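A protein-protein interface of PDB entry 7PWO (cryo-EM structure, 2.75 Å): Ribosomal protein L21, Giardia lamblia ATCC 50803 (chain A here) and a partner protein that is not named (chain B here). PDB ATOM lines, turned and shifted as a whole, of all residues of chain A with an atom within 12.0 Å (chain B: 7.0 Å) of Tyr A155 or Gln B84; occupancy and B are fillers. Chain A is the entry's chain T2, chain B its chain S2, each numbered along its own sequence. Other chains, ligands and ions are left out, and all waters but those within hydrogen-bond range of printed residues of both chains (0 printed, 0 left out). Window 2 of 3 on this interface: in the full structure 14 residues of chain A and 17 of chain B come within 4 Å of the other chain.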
ATOM      1  N   THR A 151     -19.300 -14.640  26.730  1.00  0.00           N
ATOM      2  CA  THR A 151     -18.247 -15.500  26.216  1.00  0.00           C
ATOM      3  C   THR A 151     -18.886 -16.787  25.729  1.00  0.00           C
ATOM      4  O   THR A 151     -19.985 -17.143  26.173  1.00  0.00           O
ATOM      5  CB  THR A 151     -17.195 -15.813  27.291  1.00  0.00           C
ATOM      6  OG1 THR A 151     -17.841 -16.137  28.532  1.00  0.00           O
ATOM      7  CG2 THR A 151     -16.233 -14.646  27.485  1.00  0.00           C
ATOM      8  N   PRO A 152     -18.223 -17.518  24.835  1.00  0.00           N
ATOM      9  CA  PRO A 152     -18.711 -18.852  24.478  1.00  0.00           C
ATOM     10  C   PRO A 152     -18.820 -19.733  25.713  1.00  0.00           C
ATOM     11  O   PRO A 152     -18.034 -19.617  26.654  1.00  0.00           O
ATOM     12  CB  PRO A 152     -17.638 -19.373  23.522  1.00  0.00           C
ATOM     13  CG  PRO A 152     -16.999 -18.141  22.969  1.00  0.00           C
ATOM     14  CD  PRO A 152     -17.069 -17.108  24.022  1.00  0.00           C
ATOM     15  N   LEU A 153     -19.819 -20.604  25.717  1.00  0.00           N
ATOM     16  CA  LEU A 153     -19.967 -21.550  26.809  1.00  0.00           C
ATOM     17  C   LEU A 153     -19.325 -22.884  26.464  1.00  0.00           C
ATOM     18  O   LEU A 153     -18.796 -23.097  25.372  1.00  0.00           O
ATOM     19  CB  LEU A 153     -21.437 -21.749  27.190  1.00  0.00           C
ATOM     20  CG  LEU A 153     -22.162 -20.698  28.040  1.00  0.00           C
ATOM     21  CD1 LEU A 153     -22.452 -19.414  27.301  1.00  0.00           C
ATOM     22  CD2 LEU A 153     -23.437 -21.294  28.618  1.00  0.00           C
ATOM     23  N   LYS A 154     -19.359 -23.781  27.437  1.00  0.00           N
ATOM     24  CA  LYS A 154     -18.797 -25.110  27.302  1.00  0.00           C
ATOM     25  C   LYS A 154     -19.823 -26.067  26.713  1.00  0.00           C
ATOM     26  O   LYS A 154     -21.028 -25.916  26.916  1.00  0.00           O
ATOM     27  CB  LYS A 154     -18.318 -25.614  28.658  1.00  0.00           C
ATOM     28  CG  LYS A 154     -19.416 -25.723  29.683  1.00  0.00           C
ATOM     29  CD  LYS A 154     -18.867 -26.164  31.012  1.00  0.00           C
ATOM     30  CE  LYS A 154     -18.237 -27.533  30.925  1.00  0.00           C
ATOM     31  NZ  LYS A 154     -18.206 -28.167  32.262  1.00  0.00           N
ATOM     32  N   TYR A 155     -19.329 -27.049  25.966  1.00  0.00           N
ATOM     33  CA  TYR A 155     -20.205 -28.052  25.379  1.00  0.00           C
ATOM     34  C   TYR A 155     -20.850 -28.886  26.473  1.00  0.00           C
ATOM     35  O   TYR A 155     -20.173 -29.374  27.380  1.00  0.00           O
ATOM     36  CB  TYR A 155     -19.426 -28.941  24.413  1.00  0.00           C
ATOM     37  CG  TYR A 155     -20.240 -30.059  23.801  1.00  0.00           C
ATOM     38  CD1 TYR A 155     -20.994 -29.858  22.657  1.00  0.00           C
ATOM     39  CD2 TYR A 155     -20.232 -31.326  24.363  1.00  0.00           C
ATOM     40  CE1 TYR A 155     -21.735 -30.884  22.111  1.00  0.00           C
ATOM     41  CE2 TYR A 155     -20.958 -32.355  23.825  1.00  0.00           C
ATOM     42  CZ  TYR A 155     -21.707 -32.134  22.698  1.00  0.00           C
ATOM     43  OH  TYR A 155     -22.433 -33.171  22.161  1.00  0.00           O
ATOM     44  N   ASP A 156     -22.164 -29.041  26.392  1.00  0.00           N
ATOM     45  CA  ASP A 156     -22.931 -29.764  27.397  1.00  0.00           C
ATOM     46  C   ASP A 156     -23.695 -30.867  26.682  1.00  0.00           C
ATOM     47  O   ASP A 156     -24.642 -30.592  25.937  1.00  0.00           O
ATOM     48  CB  ASP A 156     -23.876 -28.829  28.143  1.00  0.00           C
ATOM     49  CG  ASP A 156     -23.156 -27.931  29.122  1.00  0.00           C
ATOM     50  OD1 ASP A 156     -22.097 -28.329  29.645  1.00  0.00           O
ATOM     51  OD2 ASP A 156     -23.661 -26.822  29.378  1.00  0.00           O
ATOM     52  N   GLY A 157     -23.278 -32.107  26.905  1.00  0.00           N
ATOM     53  CA  GLY A 157     -23.852 -33.244  26.222  1.00  0.00           C
ATOM     54  C   GLY A 157     -23.525 -34.554  26.913  1.00  0.00           C
ATOM     55  O   GLY A 157     -22.387 -34.801  27.301  1.00  0.00           O
ATOM     56  N   LEU B  76     -11.007 -24.193  25.953  1.00  0.00           N
ATOM     57  CA  LEU B  76     -11.569 -24.119  24.616  1.00  0.00           C
ATOM     58  C   LEU B  76     -12.472 -25.315  24.349  1.00  0.00           C
ATOM     59  O   LEU B  76     -12.531 -26.274  25.123  1.00  0.00           O
ATOM     60  CB  LEU B  76     -10.457 -24.035  23.559  1.00  0.00           C
ATOM     61  CG  LEU B  76      -9.459 -25.192  23.456  1.00  0.00           C
ATOM     62  CD1 LEU B  76      -9.964 -26.367  22.625  1.00  0.00           C
ATOM     63  CD2 LEU B  76      -8.175 -24.665  22.870  1.00  0.00           C
ATOM     64  N   ARG B  77     -13.184 -25.239  23.230  1.00  0.00           N
ATOM     65  CA  ARG B  77     -13.922 -26.369  22.684  1.00  0.00           C
ATOM     66  C   ARG B  77     -13.667 -26.432  21.186  1.00  0.00           C
ATOM     67  O   ARG B  77     -13.563 -25.399  20.524  1.00  0.00           O
ATOM     68  CB  ARG B  77     -15.425 -26.271  22.979  1.00  0.00           C
ATOM     69  CG  ARG B  77     -16.106 -25.008  22.485  1.00  0.00           C
ATOM     70  CD  ARG B  77     -17.569 -24.947  22.925  1.00  0.00           C
ATOM     71  NE  ARG B  77     -18.477 -25.595  21.981  1.00  0.00           N
ATOM     72  CZ  ARG B  77     -19.797 -25.666  22.131  1.00  0.00           C
ATOM     73  NH1 ARG B  77     -20.377 -25.131  23.193  1.00  0.00           N
ATOM     74  NH2 ARG B  77     -20.541 -26.269  21.219  1.00  0.00           N
ATOM     75  N   TYR B  78     -13.545 -27.642  20.653  1.00  0.00           N
ATOM     76  CA  TYR B  78     -13.271 -27.835  19.236  1.00  0.00           C
ATOM     77  C   TYR B  78     -14.240 -28.881  18.705  1.00  0.00           C
ATOM     78  O   TYR B  78     -15.046 -29.436  19.448  1.00  0.00           O
ATOM     79  CB  TYR B  78     -11.816 -28.263  19.018  1.00  0.00           C
ATOM     80  CG  TYR B  78     -11.493 -29.599  19.618  1.00  0.00           C
ATOM     81  CD1 TYR B  78     -11.057 -29.708  20.924  1.00  0.00           C
ATOM     82  CD2 TYR B  78     -11.518 -30.745  18.844  1.00  0.00           C
ATOM     83  CE1 TYR B  78     -10.750 -30.929  21.468  1.00  0.00           C
ATOM     84  CE2 TYR B  78     -11.197 -31.961  19.372  1.00  0.00           C
ATOM     85  CZ  TYR B  78     -10.815 -32.052  20.685  1.00  0.00           C
ATOM     86  OH  TYR B  78     -10.489 -33.272  21.215  1.00  0.00           O
ATOM     87  N   ARG B  79     -14.162 -29.158  17.407  1.00  0.00           N
ATOM     88  CA  ARG B  79     -15.002 -30.173  16.784  1.00  0.00           C
ATOM     89  C   ARG B  79     -14.146 -31.162  16.007  1.00  0.00           C
ATOM     90  O   ARG B  79     -13.280 -30.760  15.227  1.00  0.00           O
ATOM     91  CB  ARG B  79     -16.050 -29.540  15.862  1.00  0.00           C
ATOM     92  CG  ARG B  79     -16.931 -30.563  15.173  1.00  0.00           C
ATOM     93  CD  ARG B  79     -17.875 -29.924  14.182  1.00  0.00           C
ATOM     94  NE  ARG B  79     -19.136 -29.513  14.782  1.00  0.00           N
ATOM     95  CZ  ARG B  79     -20.206 -30.298  14.870  1.00  0.00           C
ATOM     96  NH1 ARG B  79     -20.161 -31.538  14.416  1.00  0.00           N
ATOM     97  NH2 ARG B  79     -21.319 -29.845  15.414  1.00  0.00           N
ATOM     98  N   SER B  80     -14.387 -32.450  16.227  1.00  0.00           N
ATOM     99  CA  SER B  80     -13.772 -33.531  15.470  1.00  0.00           C
ATOM    100  C   SER B  80     -14.837 -34.233  14.634  1.00  0.00           C
ATOM    101  O   SER B  80     -15.994 -33.826  14.592  1.00  0.00           O
ATOM    102  CB  SER B  80     -13.069 -34.522  16.401  1.00  0.00           C
ATOM    103  OG  SER B  80     -13.981 -35.469  16.943  1.00  0.00           O
ATOM    104  N   VAL B  82     -16.283 -36.995  15.222  1.00  0.00           N
ATOM    105  CA  VAL B  82     -17.211 -37.840  15.966  1.00  0.00           C
ATOM    106  C   VAL B  82     -18.062 -37.019  16.929  1.00  0.00           C
ATOM    107  O   VAL B  82     -19.003 -37.544  17.532  1.00  0.00           O
ATOM    108  CB  VAL B  82     -16.472 -38.955  16.733  1.00  0.00           C
ATOM    109  CG1 VAL B  82     -15.736 -39.886  15.782  1.00  0.00           C
ATOM    110  CG2 VAL B  82     -15.518 -38.355  17.751  1.00  0.00           C
ATOM    111  N   GLY B  83     -17.742 -35.744  17.103  1.00  0.00           N
ATOM    112  CA  GLY B  83     -18.478 -34.949  18.068  1.00  0.00           C
ATOM    113  C   GLY B  83     -17.716 -33.694  18.451  1.00  0.00           C
ATOM    114  O   GLY B  83     -16.853 -33.227  17.716  1.00  0.00           O
ATOM    115  N   GLN B  84     -18.073 -33.166  19.618  1.00  0.00           N
ATOM    116  CA  GLN B  84     -17.471 -31.969  20.181  1.00  0.00           C
ATOM    117  C   GLN B  84     -16.896 -32.279  21.557  1.00  0.00           C
ATOM    118  O   GLN B  84     -17.419 -33.128  22.284  1.00  0.00           O
ATOM    119  CB  GLN B  84     -18.501 -30.840  20.279  1.00  0.00           C
ATOM    120  CG  GLN B  84     -18.823 -30.198  18.953  1.00  0.00           C
ATOM    121  CD  GLN B  84     -20.201 -29.613  18.910  1.00  0.00           C
ATOM    122  OE1 GLN B  84     -21.183 -30.298  19.182  1.00  0.00           O
ATOM    123  NE2 GLN B  84     -20.288 -28.333  18.590  1.00  0.00           N
ATOM    124  N   HIS B  85     -15.815 -31.585  21.910  1.00  0.00           N
ATOM    125  CA  HIS B  85     -15.080 -31.869  23.135  1.00  0.00           C
ATOM    126  C   HIS B  85     -14.609 -30.573  23.780  1.00  0.00           C
ATOM    127  O   HIS B  85     -14.509 -29.533  23.132  1.00  0.00           O
ATOM    128  CB  HIS B  85     -13.888 -32.793  22.854  1.00  0.00           C
ATOM    129  CG  HIS B  85     -14.235 -33.980  22.010  1.00  0.00           C
ATOM    130  ND1 HIS B  85     -14.321 -33.920  20.637  1.00  0.00           N
ATOM    131  CD2 HIS B  85     -14.552 -35.251  22.349  1.00  0.00           C
ATOM    132  CE1 HIS B  85     -14.659 -35.106  20.165  1.00  0.00           C
ATOM    133  NE2 HIS B  85     -14.805 -35.931  21.183  1.00  0.00           N
ATOM    134  N   ASN B  86     -14.329 -30.649  25.077  1.00  0.00           N
ATOM    135  CA  ASN B  86     -13.791 -29.541  25.857  1.00  0.00           C
ATOM    136  C   ASN B  86     -12.334 -29.823  26.195  1.00  0.00           C
ATOM    137  O   ASN B  86     -11.939 -30.978  26.356  1.00  0.00           O
ATOM    138  CB  ASN B  86     -14.595 -29.326  27.145  1.00  0.00           C
ATOM    139  CG  ASN B  86     -15.979 -28.769  26.893  1.00  0.00           C
ATOM    140  OD1 ASN B  86     -16.959 -29.502  26.833  1.00  0.00           O
ATOM    141  ND2 ASN B  86     -16.065 -27.454  26.762  1.00  0.00           N
ATOM    142  N   ASP B 117     -13.044 -24.068  13.603  1.00  0.00           N
ATOM    143  CA  ASP B 117     -13.514 -25.272  14.259  1.00  0.00           C
ATOM    144  C   ASP B 117     -13.537 -25.130  15.771  1.00  0.00           C
ATOM    145  O   ASP B 117     -14.068 -26.011  16.453  1.00  0.00           O
ATOM    146  CB  ASP B 117     -12.603 -26.440  13.876  1.00  0.00           C
ATOM    147  CG  ASP B 117     -12.739 -26.815  12.426  1.00  0.00           C
ATOM    148  OD1 ASP B 117     -13.836 -26.616  11.866  1.00  0.00           O
ATOM    149  OD2 ASP B 117     -11.740 -27.273  11.832  1.00  0.00           O
ATOM    150  N   GLN B 119     -13.837 -22.757  19.437  1.00  0.00           N
ATOM    151  CA  GLN B 119     -14.363 -21.611  20.172  1.00  0.00           C
ATOM    152  C   GLN B 119     -13.624 -21.497  21.496  1.00  0.00           C
ATOM    153  O   GLN B 119     -13.511 -22.478  22.233  1.00  0.00           O
ATOM    154  CB  GLN B 119     -15.873 -21.726  20.427  1.00  0.00           C
ATOM    155  CG  GLN B 119     -16.694 -22.247  19.252  1.00  0.00           C
ATOM    156  CD  GLN B 119     -18.157 -22.478  19.611  1.00  0.00           C
ATOM    157  OE1 GLN B 119     -18.667 -21.916  20.575  1.00  0.00           O
ATOM    158  NE2 GLN B 119     -18.832 -23.318  18.835  1.00  0.00           N
ATOM    159  N   ILE B 121     -13.373 -20.391  25.182  1.00  0.00           N
ATOM    160  CA  ILE B 121     -14.125 -19.967  26.360  1.00  0.00           C
ATOM    161  C   ILE B 121     -13.313 -18.985  27.195  1.00  0.00           C
ATOM    162  O   ILE B 121     -13.739 -17.850  27.430  1.00  0.00           O
ATOM    163  CB  ILE B 121     -14.581 -21.176  27.202  1.00  0.00           C
ATOM    164  CG1 ILE B 121     -15.548 -22.082  26.436  1.00  0.00           C
ATOM    165  CG2 ILE B 121     -15.210 -20.719  28.489  1.00  0.00           C
ATOM    166  CD1 ILE B 121     -14.920 -23.150  25.640  1.00  0.00           C
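Tyr A155 touches just these residues of chain B: Arg B77, Gln B84 and Asn B86. Gln B84 touches just one residue of chain A: Tyr A155 (3.0 Å). Of chain A, only Leu A153, Lys A154 and Tyr A155 come within 4 Å of Arg B77. Tyr B78 touches none of the printed residues of chain A. No residue of chain A comes within 4 Å of Arg B79. No residue of chain A comes within 4 Å of Ser B80. No residue of chain A comes within 4 Å of Gly B83. No residue of chain A comes within 4 Å of His B85. Printed residues of chain B within 4 Å of Lys A154: Arg B77 (3.7 Å) and Asn B86 (3.5 Å). Printed residues of chain B within 4 Å of Pro A152: Ile B121 (3.5 Å). Printed residues of chain B within 4 Å of Leu A153: Arg B77 (3.3 Å) and Ile B121 (3.6 Å). Of the printed residues of chain A, Ile B121 touches Pro A152 and Leu A153. The nearest printed residue of chain A that does not touch Ile B121 is Thr A151 (4.01 Å).
NE2 of Gln B84 lies close to NH2 of Arg B77 (3.4 Å). The backbone carbonyl oxygen (O) of Arg B77 sits at hydrogen-bond distance from the backbone NH (N) of Gln B119 (2.9 Å).
CG1 of Ile B121 touches O of Pro A152, at 3.5 Å. CG1 of Ile B121 touches O of Leu A153 (3.6 Å). Lys A154 touches Arg B77. Lys A154 touches Asn B86. Tyr A155 touches Arg B77 (N to NH1, 3.5 Å). Gln B84 touches Tyr A155 (OE1 to CE1, 3.0 Å).
The guanidinium group of Arg B77 sits close to the backbone carbonyl oxygen of Leu A153 (3.4 Å). The backbone carbonyl oxygen of Tyr A155 sits close to the side-chain amide oxygen of Asn B86, 3.3 Å away.
Of the 7 printed residues of chain A, 4 touch a printed residue of chain B. Printed residues of chain A that touch a printed residue of chain B: Pro A152, Leu A153, Lys A154 and Tyr A155. Along chain A the printed residues that touch a printed residue of chain B span positions 152 to 155. Of the 13 printed residues of chain B, 4 touch a printed residue of chain A. Hydrophobic or aromatic side chains of chain B within 4 Å of the printed part of chain A: Ile B121. Among the printed residues, no Asp or Glu carboxylate lies within 4 Å of a Lys or Arg side-chain nitrogen of the other chain.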
